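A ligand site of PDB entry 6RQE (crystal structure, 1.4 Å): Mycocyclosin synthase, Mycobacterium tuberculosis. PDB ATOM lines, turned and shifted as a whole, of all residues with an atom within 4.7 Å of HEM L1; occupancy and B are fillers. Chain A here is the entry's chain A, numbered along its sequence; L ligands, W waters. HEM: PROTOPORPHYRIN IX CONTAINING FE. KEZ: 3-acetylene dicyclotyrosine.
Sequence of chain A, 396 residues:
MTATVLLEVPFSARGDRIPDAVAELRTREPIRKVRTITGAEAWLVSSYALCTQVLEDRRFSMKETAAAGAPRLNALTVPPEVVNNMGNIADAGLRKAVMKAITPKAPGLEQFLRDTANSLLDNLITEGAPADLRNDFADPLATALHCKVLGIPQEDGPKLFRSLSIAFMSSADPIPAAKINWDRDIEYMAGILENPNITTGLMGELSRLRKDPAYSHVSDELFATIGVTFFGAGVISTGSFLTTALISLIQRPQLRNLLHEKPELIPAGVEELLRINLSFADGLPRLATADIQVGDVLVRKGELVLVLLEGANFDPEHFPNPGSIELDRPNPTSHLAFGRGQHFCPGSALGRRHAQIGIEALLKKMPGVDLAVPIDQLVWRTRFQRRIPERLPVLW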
ATOM      1  N   MET A  62     -39.639  -4.594 -16.590  1.00  0.00           N
ATOM      2  CA  MET A  62     -39.437  -5.620 -17.602  1.00  0.00           C
ATOM      3  C   MET A  62     -40.790  -6.050 -18.179  1.00  0.00           C
ATOM      4  O   MET A  62     -40.977  -6.134 -19.406  1.00  0.00           O
ATOM      5  CB  MET A  62     -38.676  -6.837 -17.042  1.00  0.00           C
ATOM      6  CG  MET A  62     -38.721  -8.095 -17.975  1.00  0.00           C
ATOM      7  SD  MET A  62     -37.941  -9.581 -17.272  1.00  0.00           S
ATOM      8  CE  MET A  62     -36.279  -9.013 -17.349  1.00  0.00           C
ATOM      9  N   MET A  86     -40.660 -14.696 -14.231  1.00  0.00           N
ATOM     10  CA  MET A  86     -40.297 -14.811 -12.818  1.00  0.00           C
ATOM     11  C   MET A  86     -41.405 -14.309 -11.896  1.00  0.00           C
ATOM     12  O   MET A  86     -41.605 -14.862 -10.817  1.00  0.00           O
ATOM     13  CB  MET A  86     -38.963 -14.129 -12.518  1.00  0.00           C
ATOM     14  CG  MET A  86     -37.725 -14.915 -12.994  1.00  0.00           C
ATOM     15  SD  MET A  86     -37.452 -16.549 -12.256  1.00  0.00           S
ATOM     16  CE  MET A  86     -37.642 -16.203 -10.501  1.00  0.00           C
ATOM     17  N   ILE A 102     -31.905 -25.311  -9.096  1.00  0.00           N
ATOM     18  CA  ILE A 102     -30.918 -24.884 -10.090  1.00  0.00           C
ATOM     19  C   ILE A 102     -29.610 -24.451  -9.429  1.00  0.00           C
ATOM     20  O   ILE A 102     -28.787 -23.797 -10.064  1.00  0.00           O
ATOM     21  CB  ILE A 102     -31.479 -23.832 -11.057  1.00  0.00           C
ATOM     22  CG1 ILE A 102     -31.802 -22.533 -10.351  1.00  0.00           C
ATOM     23  CG2 ILE A 102     -32.713 -24.398 -11.778  1.00  0.00           C
ATOM     24  CD1 ILE A 102     -32.143 -21.406 -11.281  1.00  0.00           C
ATOM     25  N   HIS A 146     -27.903 -28.760 -18.385  1.00  0.00           N
ATOM     26  CA  HIS A 146     -29.298 -28.378 -18.187  1.00  0.00           C
ATOM     27  C   HIS A 146     -30.232 -29.567 -18.257  1.00  0.00           C
ATOM     28  O   HIS A 146     -31.242 -29.586 -17.536  1.00  0.00           O
ATOM     29  CB  HIS A 146     -29.677 -27.217 -19.089  1.00  0.00           C
ATOM     30  CG  HIS A 146     -29.117 -25.932 -18.614  1.00  0.00           C
ATOM     31  ND1 HIS A 146     -27.799 -25.576 -18.825  1.00  0.00           N
ATOM     32  CD2 HIS A 146     -29.649 -24.953 -17.835  1.00  0.00           C
ATOM     33  CE1 HIS A 146     -27.564 -24.425 -18.237  1.00  0.00           C
ATOM     34  NE2 HIS A 146     -28.663 -24.021 -17.625  1.00  0.00           N
ATOM     35  N   PHE A 230     -36.287 -22.172 -18.558  1.00  0.00           N
ATOM     36  CA  PHE A 230     -35.043 -22.371 -17.818  1.00  0.00           C
ATOM     37  C   PHE A 230     -34.036 -23.164 -18.651  1.00  0.00           C
ATOM     38  O   PHE A 230     -32.847 -22.865 -18.634  1.00  0.00           O
ATOM     39  CB  PHE A 230     -35.323 -22.952 -16.420  1.00  0.00           C
ATOM     40  CG  PHE A 230     -35.646 -21.891 -15.402  1.00  0.00           C
ATOM     41  CD1 PHE A 230     -36.823 -21.153 -15.502  1.00  0.00           C
ATOM     42  CD2 PHE A 230     -34.733 -21.555 -14.397  1.00  0.00           C
ATOM     43  CE1 PHE A 230     -37.123 -20.143 -14.605  1.00  0.00           C
ATOM     44  CE2 PHE A 230     -35.033 -20.545 -13.501  1.00  0.00           C
ATOM     45  CZ  PHE A 230     -36.219 -19.847 -13.605  1.00  0.00           C
ATOM     46  N   ALA A 233     -32.963 -20.311 -21.547  1.00  0.00           N
ATOM     47  CA  ALA A 233     -32.166 -19.208 -21.020  1.00  0.00           C
ATOM     48  C   ALA A 233     -30.860 -19.719 -20.442  1.00  0.00           C
ATOM     49  O   ALA A 233     -29.790 -19.125 -20.642  1.00  0.00           O
ATOM     50  CB  ALA A 233     -32.955 -18.427 -19.972  1.00  0.00           C
ATOM     51  N   GLY A 234     -30.916 -20.826 -19.718  1.00  0.00           N
ATOM     52  CA  GLY A 234     -29.706 -21.344 -19.104  1.00  0.00           C
ATOM     53  C   GLY A 234     -28.703 -21.826 -20.145  1.00  0.00           C
ATOM     54  O   GLY A 234     -27.515 -21.513 -20.075  1.00  0.00           O
ATOM     55  N   SER A 237     -27.293 -18.960 -22.278  1.00  0.00           N
ATOM     56  CA  SER A 237     -26.487 -18.015 -21.542  1.00  0.00           C
ATOM     57  C   SER A 237     -25.160 -18.642 -21.116  1.00  0.00           C
ATOM     58  O   SER A 237     -24.112 -18.013 -21.246  1.00  0.00           O
ATOM     59  CB  SER A 237     -27.218 -17.488 -20.309  1.00  0.00           C
ATOM     60  OG  SER A 237     -28.402 -16.794 -20.701  1.00  0.00           O
ATOM     61  N   THR A 238     -25.192 -19.883 -20.619  1.00  0.00           N
ATOM     62  CA  THR A 238     -23.945 -20.543 -20.219  1.00  0.00           C
ATOM     63  C   THR A 238     -23.106 -20.937 -21.422  1.00  0.00           C
ATOM     64  O   THR A 238     -21.883 -20.760 -21.403  1.00  0.00           O
ATOM     65  CB  THR A 238     -24.222 -21.762 -19.344  1.00  0.00           C
ATOM     66  OG1 THR A 238     -25.037 -22.719 -20.014  1.00  0.00           O
ATOM     67  CG2 THR A 238     -24.873 -21.375 -18.039  1.00  0.00           C
ATOM     68  N   PHE A 241     -21.662 -17.625 -22.846  1.00  0.00           N
ATOM     69  CA  PHE A 241     -20.670 -17.044 -21.968  1.00  0.00           C
ATOM     70  C   PHE A 241     -19.385 -17.848 -21.987  1.00  0.00           C
ATOM     71  O   PHE A 241     -18.290 -17.306 -22.127  1.00  0.00           O
ATOM     72  CB  PHE A 241     -21.154 -16.896 -20.515  1.00  0.00           C
ATOM     73  CG  PHE A 241     -20.043 -16.559 -19.614  1.00  0.00           C
ATOM     74  CD1 PHE A 241     -19.384 -15.373 -19.761  1.00  0.00           C
ATOM     75  CD2 PHE A 241     -19.594 -17.459 -18.668  1.00  0.00           C
ATOM     76  CE1 PHE A 241     -18.267 -15.073 -19.004  1.00  0.00           C
ATOM     77  CE2 PHE A 241     -18.493 -17.160 -17.895  1.00  0.00           C
ATOM     78  CZ  PHE A 241     -17.825 -15.986 -18.074  1.00  0.00           C
ATOM     79  N   LEU A 274     -16.510 -12.898 -16.565  1.00  0.00           N
ATOM     80  CA  LEU A 274     -17.883 -12.407 -16.528  1.00  0.00           C
ATOM     81  C   LEU A 274     -17.921 -10.904 -16.689  1.00  0.00           C
ATOM     82  O   LEU A 274     -18.719 -10.366 -17.483  1.00  0.00           O
ATOM     83  CB  LEU A 274     -18.546 -12.815 -15.223  1.00  0.00           C
ATOM     84  CG  LEU A 274     -18.984 -14.277 -15.143  1.00  0.00           C
ATOM     85  CD1 LEU A 274     -19.236 -14.688 -13.686  1.00  0.00           C
ATOM     86  CD2 LEU A 274     -20.255 -14.478 -15.980  1.00  0.00           C
ATOM     87  N   SER A 279     -21.264 -11.191 -24.117  1.00  0.00           N
ATOM     88  CA  SER A 279     -22.241 -12.168 -24.601  1.00  0.00           C
ATOM     89  C   SER A 279     -23.619 -11.551 -24.869  1.00  0.00           C
ATOM     90  O   SER A 279     -24.305 -11.970 -25.808  1.00  0.00           O
ATOM     91  CB  SER A 279     -22.364 -13.379 -23.665  1.00  0.00           C
ATOM     92  OG  SER A 279     -23.077 -13.121 -22.470  1.00  0.00           O
ATOM     93  N   PHE A 280     -24.092 -10.599 -24.063  1.00  0.00           N
ATOM     94  CA  PHE A 280     -25.385  -9.984 -24.334  1.00  0.00           C
ATOM     95  C   PHE A 280     -25.263  -9.000 -25.465  1.00  0.00           C
ATOM     96  O   PHE A 280     -24.521  -8.025 -25.381  1.00  0.00           O
ATOM     97  CB  PHE A 280     -25.993  -9.332 -23.090  1.00  0.00           C
ATOM     98  CG  PHE A 280     -26.779 -10.297 -22.246  1.00  0.00           C
ATOM     99  CD1 PHE A 280     -26.137 -11.335 -21.591  1.00  0.00           C
ATOM    100  CD2 PHE A 280     -28.150 -10.168 -22.103  1.00  0.00           C
ATOM    101  CE1 PHE A 280     -26.873 -12.231 -20.820  1.00  0.00           C
ATOM    102  CE2 PHE A 280     -28.875 -11.057 -21.332  1.00  0.00           C
ATOM    103  CZ  PHE A 280     -28.241 -12.082 -20.704  1.00  0.00           C
ATOM    104  N   LEU A 284     -30.239  -4.438 -21.875  1.00  0.00           N
ATOM    105  CA  LEU A 284     -31.405  -5.035 -21.262  1.00  0.00           C
ATOM    106  C   LEU A 284     -32.571  -4.062 -21.348  1.00  0.00           C
ATOM    107  O   LEU A 284     -32.409  -2.901 -20.962  1.00  0.00           O
ATOM    108  CB  LEU A 284     -31.118  -5.349 -19.792  1.00  0.00           C
ATOM    109  CG  LEU A 284     -29.908  -6.245 -19.501  1.00  0.00           C
ATOM    110  CD1 LEU A 284     -29.832  -6.487 -17.994  1.00  0.00           C
ATOM    111  CD2 LEU A 284     -30.009  -7.560 -20.239  1.00  0.00           C
ATOM    112  N   ARG A 286     -36.192  -2.164 -20.639  1.00  0.00           N
ATOM    113  CA  ARG A 286     -37.169  -1.806 -19.617  1.00  0.00           C
ATOM    114  C   ARG A 286     -38.060  -0.689 -20.162  1.00  0.00           C
ATOM    115  O   ARG A 286     -37.607   0.129 -20.966  1.00  0.00           O
ATOM    116  CB  ARG A 286     -36.447  -1.242 -18.383  1.00  0.00           C
ATOM    117  CG  ARG A 286     -35.482  -2.195 -17.682  1.00  0.00           C
ATOM    118  CD  ARG A 286     -36.224  -3.325 -17.085  1.00  0.00           C
ATOM    119  NE  ARG A 286     -35.359  -4.143 -16.189  1.00  0.00           N
ATOM    120  CZ  ARG A 286     -34.690  -5.233 -16.547  1.00  0.00           C
ATOM    121  NH1 ARG A 286     -34.730  -5.688 -17.795  1.00  0.00           N
ATOM    122  NH2 ARG A 286     -33.985  -5.901 -15.627  1.00  0.00           N
ATOM    123  N   LEU A 309     -24.866  -3.503 -20.717  1.00  0.00           N
ATOM    124  CA  LEU A 309     -24.078  -4.156 -19.665  1.00  0.00           C
ATOM    125  C   LEU A 309     -22.591  -3.856 -19.803  1.00  0.00           C
ATOM    126  O   LEU A 309     -21.914  -3.610 -18.782  1.00  0.00           O
ATOM    127  CB  LEU A 309     -24.337  -5.651 -19.641  1.00  0.00           C
ATOM    128  CG  LEU A 309     -25.761  -6.105 -19.320  1.00  0.00           C
ATOM    129  CD1 LEU A 309     -25.853  -7.600 -19.311  1.00  0.00           C
ATOM    130  CD2 LEU A 309     -26.286  -5.492 -18.038  1.00  0.00           C
ATOM    131  N   LEU A 336     -22.208  -6.235 -13.708  1.00  0.00           N
ATOM    132  CA  LEU A 336     -23.616  -6.440 -14.039  1.00  0.00           C
ATOM    133  C   LEU A 336     -23.820  -7.603 -15.007  1.00  0.00           C
ATOM    134  O   LEU A 336     -24.848  -7.672 -15.683  1.00  0.00           O
ATOM    135  CB  LEU A 336     -24.223  -5.164 -14.616  1.00  0.00           C
ATOM    136  CG  LEU A 336     -24.079  -3.917 -13.763  1.00  0.00           C
ATOM    137  CD1 LEU A 336     -24.937  -2.813 -14.358  1.00  0.00           C
ATOM    138  CD2 LEU A 336     -24.463  -4.105 -12.324  1.00  0.00           C
ATOM    139  N   ALA A 337     -22.896  -8.551 -15.089  1.00  0.00           N
ATOM    140  CA  ALA A 337     -23.051  -9.647 -16.040  1.00  0.00           C
ATOM    141  C   ALA A 337     -24.287 -10.483 -15.801  1.00  0.00           C
ATOM    142  O   ALA A 337     -24.850 -11.045 -16.751  1.00  0.00           O
ATOM    143  CB  ALA A 337     -21.801 -10.543 -16.023  1.00  0.00           C
ATOM    144  N   PHE A 338     -24.784 -10.571 -14.567  1.00  0.00           N
ATOM    145  CA  PHE A 338     -26.006 -11.281 -14.229  1.00  0.00           C
ATOM    146  C   PHE A 338     -27.165 -10.329 -13.996  1.00  0.00           C
ATOM    147  O   PHE A 338     -28.206 -10.739 -13.447  1.00  0.00           O
ATOM    148  CB  PHE A 338     -25.777 -12.131 -12.968  1.00  0.00           C
ATOM    149  CG  PHE A 338     -24.808 -13.260 -13.169  1.00  0.00           C
ATOM    150  CD1 PHE A 338     -25.091 -14.297 -14.055  1.00  0.00           C
ATOM    151  CD2 PHE A 338     -23.634 -13.332 -12.441  1.00  0.00           C
ATOM    152  CE1 PHE A 338     -24.198 -15.342 -14.208  1.00  0.00           C
ATOM    153  CE2 PHE A 338     -22.772 -14.395 -12.581  1.00  0.00           C
ATOM    154  CZ  PHE A 338     -23.049 -15.401 -13.466  1.00  0.00           C
ATOM    155  N   GLY A 339     -27.021  -9.080 -14.396  1.00  0.00           N
ATOM    156  CA  GLY A 339     -28.009  -8.055 -14.112  1.00  0.00           C
ATOM    157  C   GLY A 339     -27.925  -7.548 -12.682  1.00  0.00           C
ATOM    158  O   GLY A 339     -26.905  -7.642 -12.011  1.00  0.00           O
ATOM    159  N   HIS A 343     -34.698  -8.476 -11.329  1.00  0.00           N
ATOM    160  CA  HIS A 343     -34.535  -9.535 -12.311  1.00  0.00           C
ATOM    161  C   HIS A 343     -33.137 -10.120 -12.353  1.00  0.00           C
ATOM    162  O   HIS A 343     -32.762 -10.743 -13.366  1.00  0.00           O
ATOM    163  CB  HIS A 343     -34.971  -9.021 -13.690  1.00  0.00           C
ATOM    164  CG  HIS A 343     -36.425  -8.680 -13.721  1.00  0.00           C
ATOM    165  ND1 HIS A 343     -37.404  -9.650 -13.745  1.00  0.00           N
ATOM    166  CD2 HIS A 343     -37.074  -7.492 -13.642  1.00  0.00           C
ATOM    167  CE1 HIS A 343     -38.602  -9.065 -13.716  1.00  0.00           C
ATOM    168  NE2 HIS A 343     -38.418  -7.757 -13.656  1.00  0.00           N
ATOM    169  N   CYS A 345     -30.191 -12.558 -12.314  1.00  0.00           N
ATOM    170  CA  CYS A 345     -30.209 -13.923 -12.803  1.00  0.00           C
ATOM    171  C   CYS A 345     -30.409 -14.942 -11.665  1.00  0.00           C
ATOM    172  O   CYS A 345     -29.570 -14.998 -10.740  1.00  0.00           O
ATOM    173  CB  CYS A 345     -28.874 -14.212 -13.499  1.00  0.00           C
ATOM    174  SG  CYS A 345     -28.778 -15.882 -14.128  1.00  0.00           S
ATOM    175  N   PRO A 346     -31.434 -15.799 -11.748  1.00  0.00           N
ATOM    176  CA  PRO A 346     -31.618 -16.831 -10.735  1.00  0.00           C
ATOM    177  C   PRO A 346     -30.635 -17.994 -10.854  1.00  0.00           C
ATOM    178  O   PRO A 346     -30.554 -18.811  -9.921  1.00  0.00           O
ATOM    179  CB  PRO A 346     -33.049 -17.305 -10.979  1.00  0.00           C
ATOM    180  CG  PRO A 346     -33.273 -17.119 -12.457  1.00  0.00           C
ATOM    181  CD  PRO A 346     -32.470 -15.856 -12.805  1.00  0.00           C
ATOM    182  N   GLY A 347     -29.914 -18.104 -11.948  1.00  0.00           N
ATOM    183  CA  GLY A 347     -28.987 -19.205 -12.159  1.00  0.00           C
ATOM    184  C   GLY A 347     -27.517 -18.796 -12.071  1.00  0.00           C
ATOM    185  O   GLY A 347     -26.648 -19.512 -12.611  1.00  0.00           O
ATOM    186  N   LEU A 350     -24.975 -21.431 -10.819  1.00  0.00           N
ATOM    187  CA  LEU A 350     -24.809 -22.507 -11.787  1.00  0.00           C
ATOM    188  C   LEU A 350     -24.001 -22.049 -12.986  1.00  0.00           C
ATOM    189  O   LEU A 350     -23.160 -22.787 -13.506  1.00  0.00           O
ATOM    190  CB  LEU A 350     -26.170 -22.974 -12.253  1.00  0.00           C
ATOM    191  CG  LEU A 350     -26.221 -24.236 -13.083  1.00  0.00           C
ATOM    192  CD1 LEU A 350     -25.660 -25.423 -12.291  1.00  0.00           C
ATOM    193  CD2 LEU A 350     -27.629 -24.521 -13.554  1.00  0.00           C
ATOM    194  N   GLY A 351     -24.225 -20.825 -13.438  1.00  0.00           N
ATOM    195  CA  GLY A 351     -23.444 -20.295 -14.540  1.00  0.00           C
ATOM    196  C   GLY A 351     -21.983 -20.137 -14.189  1.00  0.00           C
ATOM    197  O   GLY A 351     -21.097 -20.481 -14.995  1.00  0.00           O
HETATM  198  CHA HEM L   1     -31.817 -13.418 -16.213  1.00  0.00           C
HETATM  199  CHB HEM L   1     -27.152 -13.467 -17.490  1.00  0.00           C
HETATM  200  CHC HEM L   1     -27.042 -18.246 -16.607  1.00  0.00           C
HETATM  201  CHD HEM L   1     -31.817 -18.228 -16.167  1.00  0.00           C
HETATM  202  C1A HEM L   1     -30.532 -12.983 -16.549  1.00  0.00           C
HETATM  203  C2A HEM L   1     -30.117 -11.632 -16.730  1.00  0.00           C
HETATM  204  C3A HEM L   1     -28.822 -11.654 -17.098  1.00  0.00           C
HETATM  205  C4A HEM L   1     -28.411 -13.009 -17.160  1.00  0.00           C
HETATM  206  CMA HEM L   1     -28.003 -10.431 -17.412  1.00  0.00           C
HETATM  207  CAA HEM L   1     -30.990 -10.391 -16.493  1.00  0.00           C
HETATM  208  CBA HEM L   1     -31.875 -10.051 -17.696  1.00  0.00           C
HETATM  209  CGA HEM L   1     -32.632  -8.781 -17.422  1.00  0.00           C
HETATM  210  O1A HEM L   1     -32.600  -8.248 -16.319  1.00  0.00           O
HETATM  211  O2A HEM L   1     -33.272  -8.230 -18.291  1.00  0.00           O
HETATM  212  C1B HEM L   1     -26.653 -14.800 -17.386  1.00  0.00           C
HETATM  213  C2B HEM L   1     -25.354 -15.242 -17.641  1.00  0.00           C
HETATM  214  C3B HEM L   1     -25.325 -16.570 -17.408  1.00  0.00           C
HETATM  215  C4B HEM L   1     -26.639 -16.958 -16.996  1.00  0.00           C
HETATM  216  CMB HEM L   1     -24.208 -14.371 -18.111  1.00  0.00           C
HETATM  217  CAB HEM L   1     -24.244 -17.542 -17.524  1.00  0.00           C
HETATM  218  CBB HEM L   1     -23.045 -17.190 -17.269  1.00  0.00           C
HETATM  219  C1C HEM L   1     -28.329 -18.706 -16.351  1.00  0.00           C
HETATM  220  C2C HEM L   1     -28.716 -20.006 -15.971  1.00  0.00           C
HETATM  221  C3C HEM L   1     -30.090 -19.994 -15.870  1.00  0.00           C
HETATM  222  C4C HEM L   1     -30.512 -18.677 -16.141  1.00  0.00           C
HETATM  223  CMC HEM L   1     -27.730 -21.132 -15.778  1.00  0.00           C
HETATM  224  CAC HEM L   1     -31.047 -21.049 -15.507  1.00  0.00           C
HETATM  225  CBC HEM L   1     -30.781 -22.289 -15.520  1.00  0.00           C
HETATM  226  C1D HEM L   1     -32.223 -16.896 -16.196  1.00  0.00           C
HETATM  227  C2D HEM L   1     -33.618 -16.515 -16.112  1.00  0.00           C
HETATM  228  C3D HEM L   1     -33.626 -15.194 -16.138  1.00  0.00           C
HETATM  229  C4D HEM L   1     -32.227 -14.752 -16.230  1.00  0.00           C
HETATM  230  CMD HEM L   1     -34.785 -17.477 -16.066  1.00  0.00           C
HETATM  231  CAD HEM L   1     -34.809 -14.300 -16.119  1.00  0.00           C
HETATM  232  CBD HEM L   1     -34.952 -13.724 -14.750  1.00  0.00           C
HETATM  233  CGD HEM L   1     -36.117 -12.805 -14.839  1.00  0.00           C
HETATM  234  O1D HEM L   1     -36.402 -12.193 -13.869  1.00  0.00           O
HETATM  235  O2D HEM L   1     -36.844 -12.623 -15.807  1.00  0.00           O
HETATM  236  NA  HEM L   1     -29.463 -13.818 -16.815  1.00  0.00           N
HETATM  237  NB  HEM L   1     -27.302 -15.827 -16.930  1.00  0.00           N
HETATM  238  NC  HEM L   1     -29.421 -17.917 -16.418  1.00  0.00           N
HETATM  239  ND  HEM L   1     -31.454 -15.817 -16.174  1.00  0.00           N
HETATM  240 FE   HEM L   1     -29.422 -15.818 -16.394  1.00  0.00          FE
HETATM  241  C02 KEZ L   2     -33.265 -13.363 -21.964  1.00  0.00           C
HETATM  242  C03 KEZ L   2     -34.358 -12.697 -22.533  1.00  0.00           C
HETATM  243  C04 KEZ L   2     -35.393 -12.301 -21.773  1.00  0.00           C
HETATM  244  C05 KEZ L   2     -35.422 -12.551 -20.397  1.00  0.00           C
HETATM  245  C06 KEZ L   2     -36.630 -12.024 -19.640  1.00  0.00           C
HETATM  246  C07 KEZ L   2     -37.782 -12.969 -19.590  1.00  0.00           C
HETATM  247  C08 KEZ L   2     -38.357 -13.408 -20.890  1.00  0.00           C
HETATM  248  C10 KEZ L   2     -37.571 -15.678 -20.380  1.00  0.00           C
HETATM  249  C11 KEZ L   2     -36.270 -16.167 -21.078  1.00  0.00           C
HETATM  250  C12 KEZ L   2     -36.490 -16.788 -22.418  1.00  0.00           C
HETATM  251  C13 KEZ L   2     -36.573 -18.165 -22.346  1.00  0.00           C
HETATM  252  C14 KEZ L   2     -36.790 -18.962 -23.483  1.00  0.00           C
HETATM  253  C15 KEZ L   2     -36.989 -18.332 -24.683  1.00  0.00           C
HETATM  254  C17 KEZ L   2     -36.925 -16.967 -24.767  1.00  0.00           C
HETATM  255  C18 KEZ L   2     -36.668 -16.193 -23.630  1.00  0.00           C
HETATM  256  C19 KEZ L   2     -37.579 -15.334 -18.919  1.00  0.00           C
HETATM  257  C23 KEZ L   2     -34.330 -13.188 -19.872  1.00  0.00           C
HETATM  258  C24 KEZ L   2     -33.265 -13.580 -20.639  1.00  0.00           C
HETATM  259  C25 KEZ L   2     -32.197 -14.232 -20.114  1.00  0.00           C
HETATM  260  C26 KEZ L   2     -31.289 -14.776 -19.663  1.00  0.00           C
HETATM  261  N09 KEZ L   2     -38.247 -14.683 -21.192  1.00  0.00           N
HETATM  262  N20 KEZ L   2     -37.654 -14.022 -18.598  1.00  0.00           N
HETATM  263  O01 KEZ L   2     -32.224 -13.729 -22.690  1.00  0.00           O
HETATM  264  O16 KEZ L   2     -37.233 -19.047 -25.752  1.00  0.00           O
HETATM  265  O21 KEZ L   2     -37.442 -16.080 -18.129  1.00  0.00           O
HETATM  266  O22 KEZ L   2     -38.865 -12.679 -21.658  1.00  0.00           O
HETATM  267  O   HOH W   1     -36.074  -7.307 -20.154  1.00  0.00           O
HETATM  268  O   HOH W   2     -33.779  -9.362 -20.615  1.00  0.00           O
HETATM  269  O   HOH W   3     -39.572 -12.445 -15.825  1.00  0.00           O
HETATM  270  O   HOH W   4     -31.303  -7.715 -13.923  1.00  0.00           O
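O2D of HEM L1 sits close to SD of Met 62 (3.6 Å). Merely in contact with HEM L1: Met 86 (3.2 Å), Ala 337 (3.3 Å), Ser 237 (3.4 Å), Gly 339 (3.4 Å), His 146 (3.5 Å), Phe 338 (3.5 Å), Pro 346 (3.5 Å), Gly 234 (3.5 Å), Phe 280 (3.6 Å), Thr 238 (3.7 Å), Leu 284 (3.7 Å), Phe 230 (3.7 Å), Gly 347 (3.7 Å), Phe 241 (3.7 Å) and Ala 233 (3.98 Å). Hydrophobic or aromatic side chains within 4 Å of HEM L1: Met 62, Met 86, His 146, Phe 230, Ala 233, Phe 241, Phe 280, Leu 284, Phe 338, His 343 and Pro 346. Of the 26 residues printed, 19 come within 4 Å of HEM L1.
The backbone NH (N) of Cys 345 lies within hydrogen-bond range of the backbone carbonyl oxygen (O) of Phe 338 (2.9 Å). The backbone carbonyl oxygen of Ala 233 sits at hydrogen-bond distance from the side-chain hydroxyl of Ser 237, 2.7 Å away. The side-chain hydroxyl (OG1) of Thr 238 lies within hydrogen-bond range of the backbone carbonyl oxygen (O) of Gly 234, at 2.8 Å. N of Gly 347 lies close to SG of Cys 345 (3.3 Å). A ring nitrogen (ND1) of His 343 lies within hydrogen-bond range of the side-chain sulfur of Met 62 (3.6 Å).
The side-chain sulfur of Cys 345 binds an iron atom (FE) of HEM L1, 2.4 Å away. ND1 of His 343 lies within hydrogen-bond range of O1D of HEM L1 (2.7 Å). NH2 of Arg 286 is in salt-bridge range of O1A of HEM L1, at 2.8 Å.
Water W3 lies within hydrogen-bond range of O2D of HEM L1 (2.7 Å), N of Met 86 (3.0 Å) and SD of Met 62 (3.6 Å). Water W4 bridges an oxygen (O1A) of HEM L1 and the backbone carbonyl oxygen (O) of His 343. Water W1 lies within hydrogen-bond range of the guanidinium group (NH1) of Arg 286 and an oxygen (O2A) of HEM L1.
A nitrogen (N20) of KEZ L2 lies within hydrogen-bond range of an oxygen (O2D) of HEM L1.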
